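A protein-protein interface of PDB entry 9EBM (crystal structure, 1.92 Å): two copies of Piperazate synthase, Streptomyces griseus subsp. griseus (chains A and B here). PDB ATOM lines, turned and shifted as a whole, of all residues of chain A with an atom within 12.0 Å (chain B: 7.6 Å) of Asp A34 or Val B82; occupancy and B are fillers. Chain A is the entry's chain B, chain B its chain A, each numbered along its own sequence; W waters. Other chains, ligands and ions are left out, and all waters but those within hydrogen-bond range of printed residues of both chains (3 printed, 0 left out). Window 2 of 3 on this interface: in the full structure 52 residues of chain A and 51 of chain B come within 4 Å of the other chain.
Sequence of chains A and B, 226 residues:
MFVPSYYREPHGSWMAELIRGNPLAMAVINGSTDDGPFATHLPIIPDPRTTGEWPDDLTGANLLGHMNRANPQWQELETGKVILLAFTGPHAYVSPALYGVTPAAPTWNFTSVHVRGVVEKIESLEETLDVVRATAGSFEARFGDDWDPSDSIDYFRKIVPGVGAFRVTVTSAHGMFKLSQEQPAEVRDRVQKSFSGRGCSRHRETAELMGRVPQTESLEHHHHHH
Printed residues of chain B within 4 Å of Val A28: Val B28. Ile A29 touches none of the printed residues of chain B. Of the printed residues of chain B, Ser A32 touches Asn B30. Asp A34 touches just one residue of chain B: Val B82. Ile B29 touches just one residue of chain A: Pro A37 (3.9 Å). Of the printed residues of chain A, Asn B30 touches Asn A30 (3.4 Å), Gly A31 (2.9 Å), Ser A32 (3.1 Å), Gly A36 (3.5 Å) and Pro A37 (3.3 Å). No residue of chain A comes within 4 Å of Gly B80. Printed residues of chain A within 4 Å of Val B82: Thr A33, Asp A34 and Gly A36. Ile B83 touches none of the printed residues of chain A. Printed residues of chain A within 4 Å of Leu B84: Ala A39 (3.5 Å). No residue of chain A comes within 4 Å of Gly B117. No residue of chain A comes within 4 Å of Val B118.
Hydrophobic or aromatic side chains of chain A that line the printed part of chain B: Val A28, Pro A37 and Ala A39. Of the 18 printed residues of chain B, 6 touch a printed residue of chain A. Hydrophobic or aromatic side chains of chain B within 4 Å of the printed part of chain A: Val B28, Val B82 and Leu B84. Among the printed residues, no Asp or Glu carboxylate lies within 4 Å of a Lys or Arg side-chain nitrogen of the other chain.
N of Asp A34 sits close to OG of Ser A32. The backbone NH (N) of Thr B171 sits at hydrogen-bond distance from the backbone carbonyl oxygen (O) of Arg B116, 2.7 Å away. The side-chain hydroxyl of Ser A32 lies within hydrogen-bond range of the backbone NH of Asp A35. The backbone carbonyl oxygen (O) of Leu B84 sits at hydrogen-bond distance from the backbone NH (N) of Val B28.
Water W2 lies within hydrogen-bond range of O of Gly A31 and ND2 of Asn B30. Water W3 bridges the backbone carbonyl oxygen of Thr A33 (2.7 Å) and the backbone NH of Val B82 (3.1 Å). Water W1 lies within hydrogen-bond range of the backbone NH (N) of Ala A39 and the guanidinium group (NH2) of Arg B116.
Val A28 touches its own counterpart, Val B28. Asn B30 touches its own counterpart, Asn A30. Positions printed for both chains: 28, 29, 30 and 76. Of the 15 pairs that touch across the chains among the printed residues, 2 have their exchanged pair printed and touching as well.
Val B28 touches Val A28. OD1 of Asn A30 touches CA of Asn B30, 3.4 Å away. Thr A33 touches Val B82 (O to CG2, 3.3 Å). Asp A34 touches Val B82 (O to CG1, 3.5 Å). Gly A36 touches Asn B30 (C to OD1, 3.5 Å). Gly A36 touches Val B82 (CA to CG2, 3.4 Å). Gly A36 touches Arg B116. CG of Pro A37 touches CG1 of Val B28 (3.5 Å). Pro A37 touches Ile B29 (CG to C, 3.9 Å). Leu B84 touches Ala A39.
O of Ser A32 lies within hydrogen-bond range of ND2 of Asn B30 (3.1 Å). NH1 of Arg B116 lies within hydrogen-bond range of O of Asp A35, 2.9 Å away. N of Pro A37 sits close to OD1 of Asn B30, 3.3 Å away. The backbone NH (N) of Gly A31 lies within hydrogen-bond range of the side-chain amide oxygen (OD1) of Asn B30 (2.9 Å). The guanidinium group (NH2) of Arg B116 sits at hydrogen-bond distance from the backbone carbonyl oxygen (O) of Pro A37 (2.6 Å).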
ATOM      1  N   VAL A  28     -19.540  18.512  -3.250  1.00  0.00           N
ATOM      2  CA  VAL A  28     -20.371  18.519  -2.055  1.00  0.00           C
ATOM      3  C   VAL A  28     -21.712  17.896  -2.395  1.00  0.00           C
ATOM      4  O   VAL A  28     -22.324  18.250  -3.407  1.00  0.00           O
ATOM      5  CB  VAL A  28     -20.586  19.946  -1.519  1.00  0.00           C
ATOM      6  CG1 VAL A  28     -21.242  19.891  -0.122  1.00  0.00           C
ATOM      7  CG2 VAL A  28     -19.261  20.702  -1.478  1.00  0.00           C
ATOM      8  N   ILE A  29     -22.181  16.996  -1.542  1.00  0.00           N
ATOM      9  CA  ILE A  29     -23.525  16.450  -1.664  1.00  0.00           C
ATOM     10  C   ILE A  29     -24.138  16.435  -0.274  1.00  0.00           C
ATOM     11  O   ILE A  29     -23.430  16.472   0.735  1.00  0.00           O
ATOM     12  CB  ILE A  29     -23.534  15.023  -2.254  1.00  0.00           C
ATOM     13  CG1 ILE A  29     -22.716  14.101  -1.352  1.00  0.00           C
ATOM     14  CG2 ILE A  29     -22.977  15.003  -3.674  1.00  0.00           C
ATOM     15  CD1 ILE A  29     -22.714  12.624  -1.846  1.00  0.00           C
ATOM     16  N   ASN A  30     -25.472  16.364  -0.238  1.00  0.00           N
ATOM     17  CA  ASN A  30     -26.189  16.208   1.024  1.00  0.00           C
ATOM     18  C   ASN A  30     -25.748  14.940   1.735  1.00  0.00           C
ATOM     19  O   ASN A  30     -25.409  13.935   1.107  1.00  0.00           O
ATOM     20  CB  ASN A  30     -27.697  16.130   0.796  1.00  0.00           C
ATOM     21  CG  ASN A  30     -28.297  17.449   0.353  1.00  0.00           C
ATOM     22  OD1 ASN A  30     -27.885  18.525   0.800  1.00  0.00           O
ATOM     23  ND2 ASN A  30     -29.295  17.369  -0.525  1.00  0.00           N
ATOM     24  N   GLY A  31     -25.780  14.987   3.065  1.00  0.00           N
ATOM     25  CA  GLY A  31     -25.604  13.806   3.886  1.00  0.00           C
ATOM     26  C   GLY A  31     -26.750  13.677   4.863  1.00  0.00           C
ATOM     27  O   GLY A  31     -27.775  14.340   4.694  1.00  0.00           O
ATOM     28  N   SER A  32     -26.608  12.840   5.887  1.00  0.00           N
ATOM     29  CA  SER A  32     -27.690  12.699   6.853  1.00  0.00           C
ATOM     30  C   SER A  32     -27.773  13.940   7.741  1.00  0.00           C
ATOM     31  O   SER A  32     -26.854  14.765   7.798  1.00  0.00           O
ATOM     32  CB  SER A  32     -27.488  11.455   7.719  1.00  0.00           C
ATOM     33  OG  SER A  32     -26.503  11.705   8.711  1.00  0.00           O
ATOM     34  N   THR A  33     -28.896  14.067   8.451  1.00  0.00           N
ATOM     35  CA  THR A  33     -29.050  15.193   9.364  1.00  0.00           C
ATOM     36  C   THR A  33     -28.015  15.145  10.485  1.00  0.00           C
ATOM     37  O   THR A  33     -27.640  16.189  11.025  1.00  0.00           O
ATOM     38  CB  THR A  33     -30.464  15.213   9.950  1.00  0.00           C
ATOM     39  OG1 THR A  33     -30.688  13.999  10.667  1.00  0.00           O
ATOM     40  CG2 THR A  33     -31.495  15.319   8.860  1.00  0.00           C
ATOM     41  N   ASP A  34     -27.528  13.951  10.838  1.00  0.00           N
ATOM     42  CA  ASP A  34     -26.535  13.858  11.906  1.00  0.00           C
ATOM     43  C   ASP A  34     -25.125  14.173  11.414  1.00  0.00           C
ATOM     44  O   ASP A  34     -24.351  14.830  12.121  1.00  0.00           O
ATOM     45  CB  ASP A  34     -26.568  12.465  12.531  1.00  0.00           C
ATOM     46  CG  ASP A  34     -27.771  12.263  13.420  1.00  0.00           C
ATOM     47  OD1 ASP A  34     -28.326  13.279  13.893  1.00  0.00           O
ATOM     48  OD2 ASP A  34     -28.158  11.096  13.639  1.00  0.00           O
ATOM     49  N   ASP A  35     -24.774  13.718  10.209  1.00  0.00           N
ATOM     50  CA  ASP A  35     -23.412  13.858   9.707  1.00  0.00           C
ATOM     51  C   ASP A  35     -23.164  15.165   8.974  1.00  0.00           C
ATOM     52  O   ASP A  35     -22.011  15.592   8.878  1.00  0.00           O
ATOM     53  CB  ASP A  35     -23.075  12.706   8.761  1.00  0.00           C
ATOM     54  CG  ASP A  35     -23.218  11.353   9.419  1.00  0.00           C
ATOM     55  OD1 ASP A  35     -23.133  11.284  10.664  1.00  0.00           O
ATOM     56  OD2 ASP A  35     -23.417  10.364   8.686  1.00  0.00           O
ATOM     57  N   GLY A  36     -24.202  15.792   8.424  1.00  0.00           N
ATOM     58  CA  GLY A  36     -24.013  16.947   7.580  1.00  0.00           C
ATOM     59  C   GLY A  36     -23.595  16.547   6.180  1.00  0.00           C
ATOM     60  O   GLY A  36     -23.498  15.360   5.855  1.00  0.00           O
ATOM     61  N   PRO A  37     -23.338  17.534   5.323  1.00  0.00           N
ATOM     62  CA  PRO A  37     -23.008  17.230   3.927  1.00  0.00           C
ATOM     63  C   PRO A  37     -21.627  16.611   3.789  1.00  0.00           C
ATOM     64  O   PRO A  37     -20.750  16.803   4.636  1.00  0.00           O
ATOM     65  CB  PRO A  37     -23.070  18.597   3.239  1.00  0.00           C
ATOM     66  CG  PRO A  37     -23.021  19.592   4.330  1.00  0.00           C
ATOM     67  CD  PRO A  37     -23.589  18.972   5.544  1.00  0.00           C
ATOM     68  N   PHE A  38     -21.448  15.857   2.701  1.00  0.00           N
ATOM     69  CA  PHE A  38     -20.149  15.300   2.324  1.00  0.00           C
ATOM     70  C   PHE A  38     -19.389  16.295   1.469  1.00  0.00           C
ATOM     71  O   PHE A  38     -19.973  16.953   0.608  1.00  0.00           O
ATOM     72  CB  PHE A  38     -20.302  14.016   1.506  1.00  0.00           C
ATOM     73  CG  PHE A  38     -20.803  12.843   2.283  1.00  0.00           C
ATOM     74  CD1 PHE A  38     -19.913  11.987   2.921  1.00  0.00           C
ATOM     75  CD2 PHE A  38     -22.158  12.565   2.341  1.00  0.00           C
ATOM     76  CE1 PHE A  38     -20.375  10.878   3.625  1.00  0.00           C
ATOM     77  CE2 PHE A  38     -22.628  11.462   3.043  1.00  0.00           C
ATOM     78  CZ  PHE A  38     -21.731  10.619   3.683  1.00  0.00           C
ATOM     79  N   ALA A  39     -18.074  16.368   1.669  1.00  0.00           N
ATOM     80  CA  ALA A  39     -17.270  17.277   0.866  1.00  0.00           C
ATOM     81  C   ALA A  39     -15.902  16.664   0.623  1.00  0.00           C
ATOM     82  O   ALA A  39     -15.238  16.238   1.578  1.00  0.00           O
ATOM     83  CB  ALA A  39     -17.117  18.646   1.553  1.00  0.00           C
ATOM     84  N   GLU A  76     -22.091   7.195  -1.128  1.00  0.00           N
ATOM     85  CA  GLU A  76     -23.306   7.996  -1.090  1.00  0.00           C
ATOM     86  C   GLU A  76     -23.644   8.609  -2.443  1.00  0.00           C
ATOM     87  O   GLU A  76     -24.815   8.918  -2.686  1.00  0.00           O
ATOM     88  CB  GLU A  76     -23.192   9.089  -0.024  1.00  0.00           C
ATOM     89  CG  GLU A  76     -23.518   8.579   1.378  1.00  0.00           C
ATOM     90  CD  GLU A  76     -25.010   8.574   1.682  1.00  0.00           C
ATOM     91  OE1 GLU A  76     -25.390   8.959   2.810  1.00  0.00           O
ATOM     92  OE2 GLU A  76     -25.803   8.179   0.801  1.00  0.00           O
ATOM     93  N   VAL B  28     -21.293  25.179   4.802  1.00  0.00           N
ATOM     94  CA  VAL B  28     -22.099  24.243   4.030  1.00  0.00           C
ATOM     95  C   VAL B  28     -23.069  23.559   4.973  1.00  0.00           C
ATOM     96  O   VAL B  28     -22.653  23.035   6.008  1.00  0.00           O
ATOM     97  CB  VAL B  28     -21.214  23.196   3.324  1.00  0.00           C
ATOM     98  CG1 VAL B  28     -22.040  22.337   2.412  1.00  0.00           C
ATOM     99  CG2 VAL B  28     -20.107  23.885   2.534  1.00  0.00           C
ATOM    100  N   ILE B  29     -24.354  23.536   4.600  1.00  0.00           N
ATOM    101  CA  ILE B  29     -25.361  22.736   5.283  1.00  0.00           C
ATOM    102  C   ILE B  29     -26.139  21.942   4.242  1.00  0.00           C
ATOM    103  O   ILE B  29     -26.182  22.303   3.062  1.00  0.00           O
ATOM    104  CB  ILE B  29     -26.335  23.595   6.121  1.00  0.00           C
ATOM    105  CG1 ILE B  29     -27.147  24.508   5.204  1.00  0.00           C
ATOM    106  CG2 ILE B  29     -25.580  24.403   7.196  1.00  0.00           C
ATOM    107  CD1 ILE B  29     -28.210  25.332   5.927  1.00  0.00           C
ATOM    108  N   ASN B  30     -26.771  20.857   4.700  1.00  0.00           N
ATOM    109  CA  ASN B  30     -27.658  20.079   3.838  1.00  0.00           C
ATOM    110  C   ASN B  30     -28.763  20.964   3.279  1.00  0.00           C
ATOM    111  O   ASN B  30     -29.217  21.909   3.932  1.00  0.00           O
ATOM    112  CB  ASN B  30     -28.322  18.926   4.600  1.00  0.00           C
ATOM    113  CG  ASN B  30     -27.357  17.830   4.992  1.00  0.00           C
ATOM    114  OD1 ASN B  30     -26.416  17.509   4.267  1.00  0.00           O
ATOM    115  ND2 ASN B  30     -27.621  17.212   6.143  1.00  0.00           N
ATOM    116  N   GLU B  76     -32.411  28.563   6.491  1.00  0.00           N
ATOM    117  CA  GLU B  76     -32.204  27.145   6.764  1.00  0.00           C
ATOM    118  C   GLU B  76     -31.301  26.900   7.958  1.00  0.00           C
ATOM    119  O   GLU B  76     -31.369  25.821   8.557  1.00  0.00           O
ATOM    120  CB  GLU B  76     -31.612  26.448   5.538  1.00  0.00           C
ATOM    121  CG  GLU B  76     -32.617  26.288   4.418  1.00  0.00           C
ATOM    122  CD  GLU B  76     -33.924  25.687   4.896  1.00  0.00           C
ATOM    123  OE1 GLU B  76     -33.908  24.516   5.351  1.00  0.00           O
ATOM    124  OE2 GLU B  76     -34.958  26.392   4.820  1.00  0.00           O
ATOM    125  N   LEU B  77     -30.447  27.854   8.306  1.00  0.00           N
ATOM    126  CA  LEU B  77     -29.733  27.748   9.565  1.00  0.00           C
ATOM    127  C   LEU B  77     -30.750  27.662  10.688  1.00  0.00           C
ATOM    128  O   LEU B  77     -31.630  28.516  10.810  1.00  0.00           O
ATOM    129  CB  LEU B  77     -28.819  28.947   9.771  1.00  0.00           C
ATOM    130  CG  LEU B  77     -27.451  29.002   9.126  1.00  0.00           C
ATOM    131  CD1 LEU B  77     -26.706  30.213   9.696  1.00  0.00           C
ATOM    132  CD2 LEU B  77     -26.696  27.707   9.390  1.00  0.00           C
ATOM    133  N   GLU B  78     -30.669  26.608  11.466  1.00  0.00           N
ATOM    134  CA  GLU B  78     -31.480  26.475  12.659  1.00  0.00           C
ATOM    135  C   GLU B  78     -30.544  26.069  13.780  1.00  0.00           C
ATOM    136  O   GLU B  78     -29.580  25.328  13.552  1.00  0.00           O
ATOM    137  CB  GLU B  78     -32.605  25.434  12.479  1.00  0.00           C
ATOM    138  N   THR B  79     -30.804  26.581  14.973  1.00  0.00           N
ATOM    139  CA  THR B  79     -30.029  26.168  16.128  1.00  0.00           C
ATOM    140  C   THR B  79     -30.113  24.651  16.278  1.00  0.00           C
ATOM    141  O   THR B  79     -31.205  24.078  16.296  1.00  0.00           O
ATOM    142  CB  THR B  79     -30.541  26.887  17.375  1.00  0.00           C
ATOM    143  OG1 THR B  79     -30.085  28.246  17.337  1.00  0.00           O
ATOM    144  CG2 THR B  79     -30.022  26.210  18.641  1.00  0.00           C
ATOM    145  N   GLY B  80     -28.952  24.001  16.344  1.00  0.00           N
ATOM    146  CA  GLY B  80     -28.870  22.559  16.440  1.00  0.00           C
ATOM    147  C   GLY B  80     -28.595  21.851  15.131  1.00  0.00           C
ATOM    148  O   GLY B  80     -28.340  20.644  15.144  1.00  0.00           O
ATOM    149  N   LYS B  81     -28.648  22.562  14.010  1.00  0.00           N
ATOM    150  CA  LYS B  81     -28.311  21.978  12.718  1.00  0.00           C
ATOM    151  C   LYS B  81     -26.805  21.762  12.628  1.00  0.00           C
ATOM    152  O   LYS B  81     -26.013  22.538  13.171  1.00  0.00           O
ATOM    153  CB  LYS B  81     -28.774  22.905  11.594  1.00  0.00           C
ATOM    154  CG  LYS B  81     -29.076  22.226  10.268  1.00  0.00           C
ATOM    155  CD  LYS B  81     -29.893  23.157   9.380  1.00  0.00           C
ATOM    156  CE  LYS B  81     -30.964  22.428   8.582  1.00  0.00           C
ATOM    157  NZ  LYS B  81     -30.437  22.022   7.236  1.00  0.00           N
ATOM    158  N   VAL B  82     -26.401  20.687  11.955  1.00  0.00           N
ATOM    159  CA  VAL B  82     -24.971  20.473  11.775  1.00  0.00           C
ATOM    160  C   VAL B  82     -24.499  21.298  10.587  1.00  0.00           C
ATOM    161  O   VAL B  82     -25.248  21.564   9.643  1.00  0.00           O
ATOM    162  CB  VAL B  82     -24.630  18.980  11.609  1.00  0.00           C
ATOM    163  CG1 VAL B  82     -25.043  18.195  12.870  1.00  0.00           C
ATOM    164  CG2 VAL B  82     -25.305  18.429  10.387  1.00  0.00           C
ATOM    165  N   ILE B  83     -23.252  21.741  10.649  1.00  0.00           N
ATOM    166  CA  ILE B  83     -22.691  22.594   9.615  1.00  0.00           C
ATOM    167  C   ILE B  83     -21.278  22.120   9.326  1.00  0.00           C
ATOM    168  O   ILE B  83     -20.614  21.522  10.181  1.00  0.00           O
ATOM    169  CB  ILE B  83     -22.719  24.075  10.045  1.00  0.00           C
ATOM    170  CG1 ILE B  83     -22.225  25.001   8.922  1.00  0.00           C
ATOM    171  CG2 ILE B  83     -21.951  24.259  11.354  1.00  0.00           C
ATOM    172  CD1 ILE B  83     -22.684  26.477   9.084  1.00  0.00           C
ATOM    173  N   LEU B  84     -20.828  22.367   8.099  1.00  0.00           N
ATOM    174  CA  LEU B  84     -19.447  22.138   7.700  1.00  0.00           C
ATOM    175  C   LEU B  84     -18.820  23.478   7.329  1.00  0.00           C
ATOM    176  O   LEU B  84     -19.403  24.260   6.571  1.00  0.00           O
ATOM    177  CB  LEU B  84     -19.355  21.155   6.523  1.00  0.00           C
ATOM    178  CG  LEU B  84     -18.054  21.240   5.710  1.00  0.00           C
ATOM    179  CD1 LEU B  84     -16.881  20.694   6.494  1.00  0.00           C
ATOM    180  CD2 LEU B  84     -18.186  20.542   4.333  1.00  0.00           C
ATOM    181  N   ARG B 116     -16.525  20.511  11.447  1.00  0.00           N
ATOM    182  CA  ARG B 116     -17.931  20.201  11.623  1.00  0.00           C
ATOM    183  C   ARG B 116     -18.368  20.603  13.017  1.00  0.00           C
ATOM    184  O   ARG B 116     -17.590  20.542  13.974  1.00  0.00           O
ATOM    185  CB  ARG B 116     -18.208  18.714  11.398  1.00  0.00           C
ATOM    186  CG  ARG B 116     -18.081  18.391   9.949  1.00  0.00           C
ATOM    187  CD  ARG B 116     -18.492  17.002   9.608  1.00  0.00           C
ATOM    188  NE  ARG B 116     -18.114  16.787   8.223  1.00  0.00           N
ATOM    189  CZ  ARG B 116     -18.929  16.958   7.193  1.00  0.00           C
ATOM    190  NH1 ARG B 116     -20.211  17.305   7.401  1.00  0.00           N
ATOM    191  NH2 ARG B 116     -18.460  16.743   5.965  1.00  0.00           N
ATOM    192  N   GLY B 117     -19.629  20.993  13.124  1.00  0.00           N
ATOM    193  CA  GLY B 117     -20.126  21.452  14.398  1.00  0.00           C
ATOM    194  C   GLY B 117     -21.612  21.712  14.335  1.00  0.00           C
ATOM    195  O   GLY B 117     -22.277  21.391  13.350  1.00  0.00           O
ATOM    196  N   VAL B 118     -22.112  22.309  15.413  1.00  0.00           N
ATOM    197  CA  VAL B 118     -23.534  22.528  15.640  1.00  0.00           C
ATOM    198  C   VAL B 118     -23.781  24.031  15.678  1.00  0.00           C
ATOM    199  O   VAL B 118     -23.079  24.758  16.389  1.00  0.00           O
ATOM    200  CB  VAL B 118     -23.985  21.845  16.941  1.00  0.00           C
ATOM    201  CG1 VAL B 118     -25.440  22.128  17.219  1.00  0.00           C
ATOM    202  CG2 VAL B 118     -23.748  20.354  16.835  1.00  0.00           C
ATOM    203  N   VAL B 119     -24.764  24.489  14.896  1.00  0.00           N
ATOM    204  CA  VAL B 119     -25.073  25.910  14.752  1.00  0.00           C
ATOM    205  C   VAL B 119     -25.893  26.410  15.935  1.00  0.00           C
ATOM    206  O   VAL B 119     -26.768  25.714  16.468  1.00  0.00           O
ATOM    207  CB  VAL B 119     -25.822  26.170  13.430  1.00  0.00           C
ATOM    208  CG1 VAL B 119     -26.187  27.635  13.296  1.00  0.00           C
ATOM    209  CG2 VAL B 119     -24.974  25.767  12.256  1.00  0.00           C
ATOM    210  N   VAL B 168     -20.786  28.416  15.975  1.00  0.00           N
ATOM    211  CA  VAL B 168     -20.632  27.001  15.659  1.00  0.00           C
ATOM    212  C   VAL B 168     -19.845  26.384  16.804  1.00  0.00           C
ATOM    213  O   VAL B 168     -18.764  26.873  17.166  1.00  0.00           O
ATOM    214  CB  VAL B 168     -19.933  26.778  14.308  1.00  0.00           C
ATOM    215  CG1 VAL B 168     -19.690  25.261  14.053  1.00  0.00           C
ATOM    216  CG2 VAL B 168     -20.746  27.378  13.168  1.00  0.00           C
ATOM    217  N   THR B 171     -17.664  20.002  16.585  1.00  0.00           N
ATOM    218  CA  THR B 171     -17.683  18.602  17.001  1.00  0.00           C
ATOM    219  C   THR B 171     -16.524  17.789  16.440  1.00  0.00           C
ATOM    220  O   THR B 171     -16.173  16.762  17.028  1.00  0.00           O
ATOM    221  CB  THR B 171     -18.995  17.926  16.590  1.00  0.00           C
ATOM    222  OG1 THR B 171     -19.233  18.190  15.207  1.00  0.00           O
ATOM    223  CG2 THR B 171     -20.167  18.452  17.432  1.00  0.00           C
HETATM  224  O   HOH W   1     -17.029  14.530   3.775  1.00  0.00           O
HETATM  225  O   HOH W   2     -30.192  15.544   4.517  1.00  0.00           O
HETATM  226  O   HOH W   3     -28.560  18.738  10.939  1.00  0.00           O
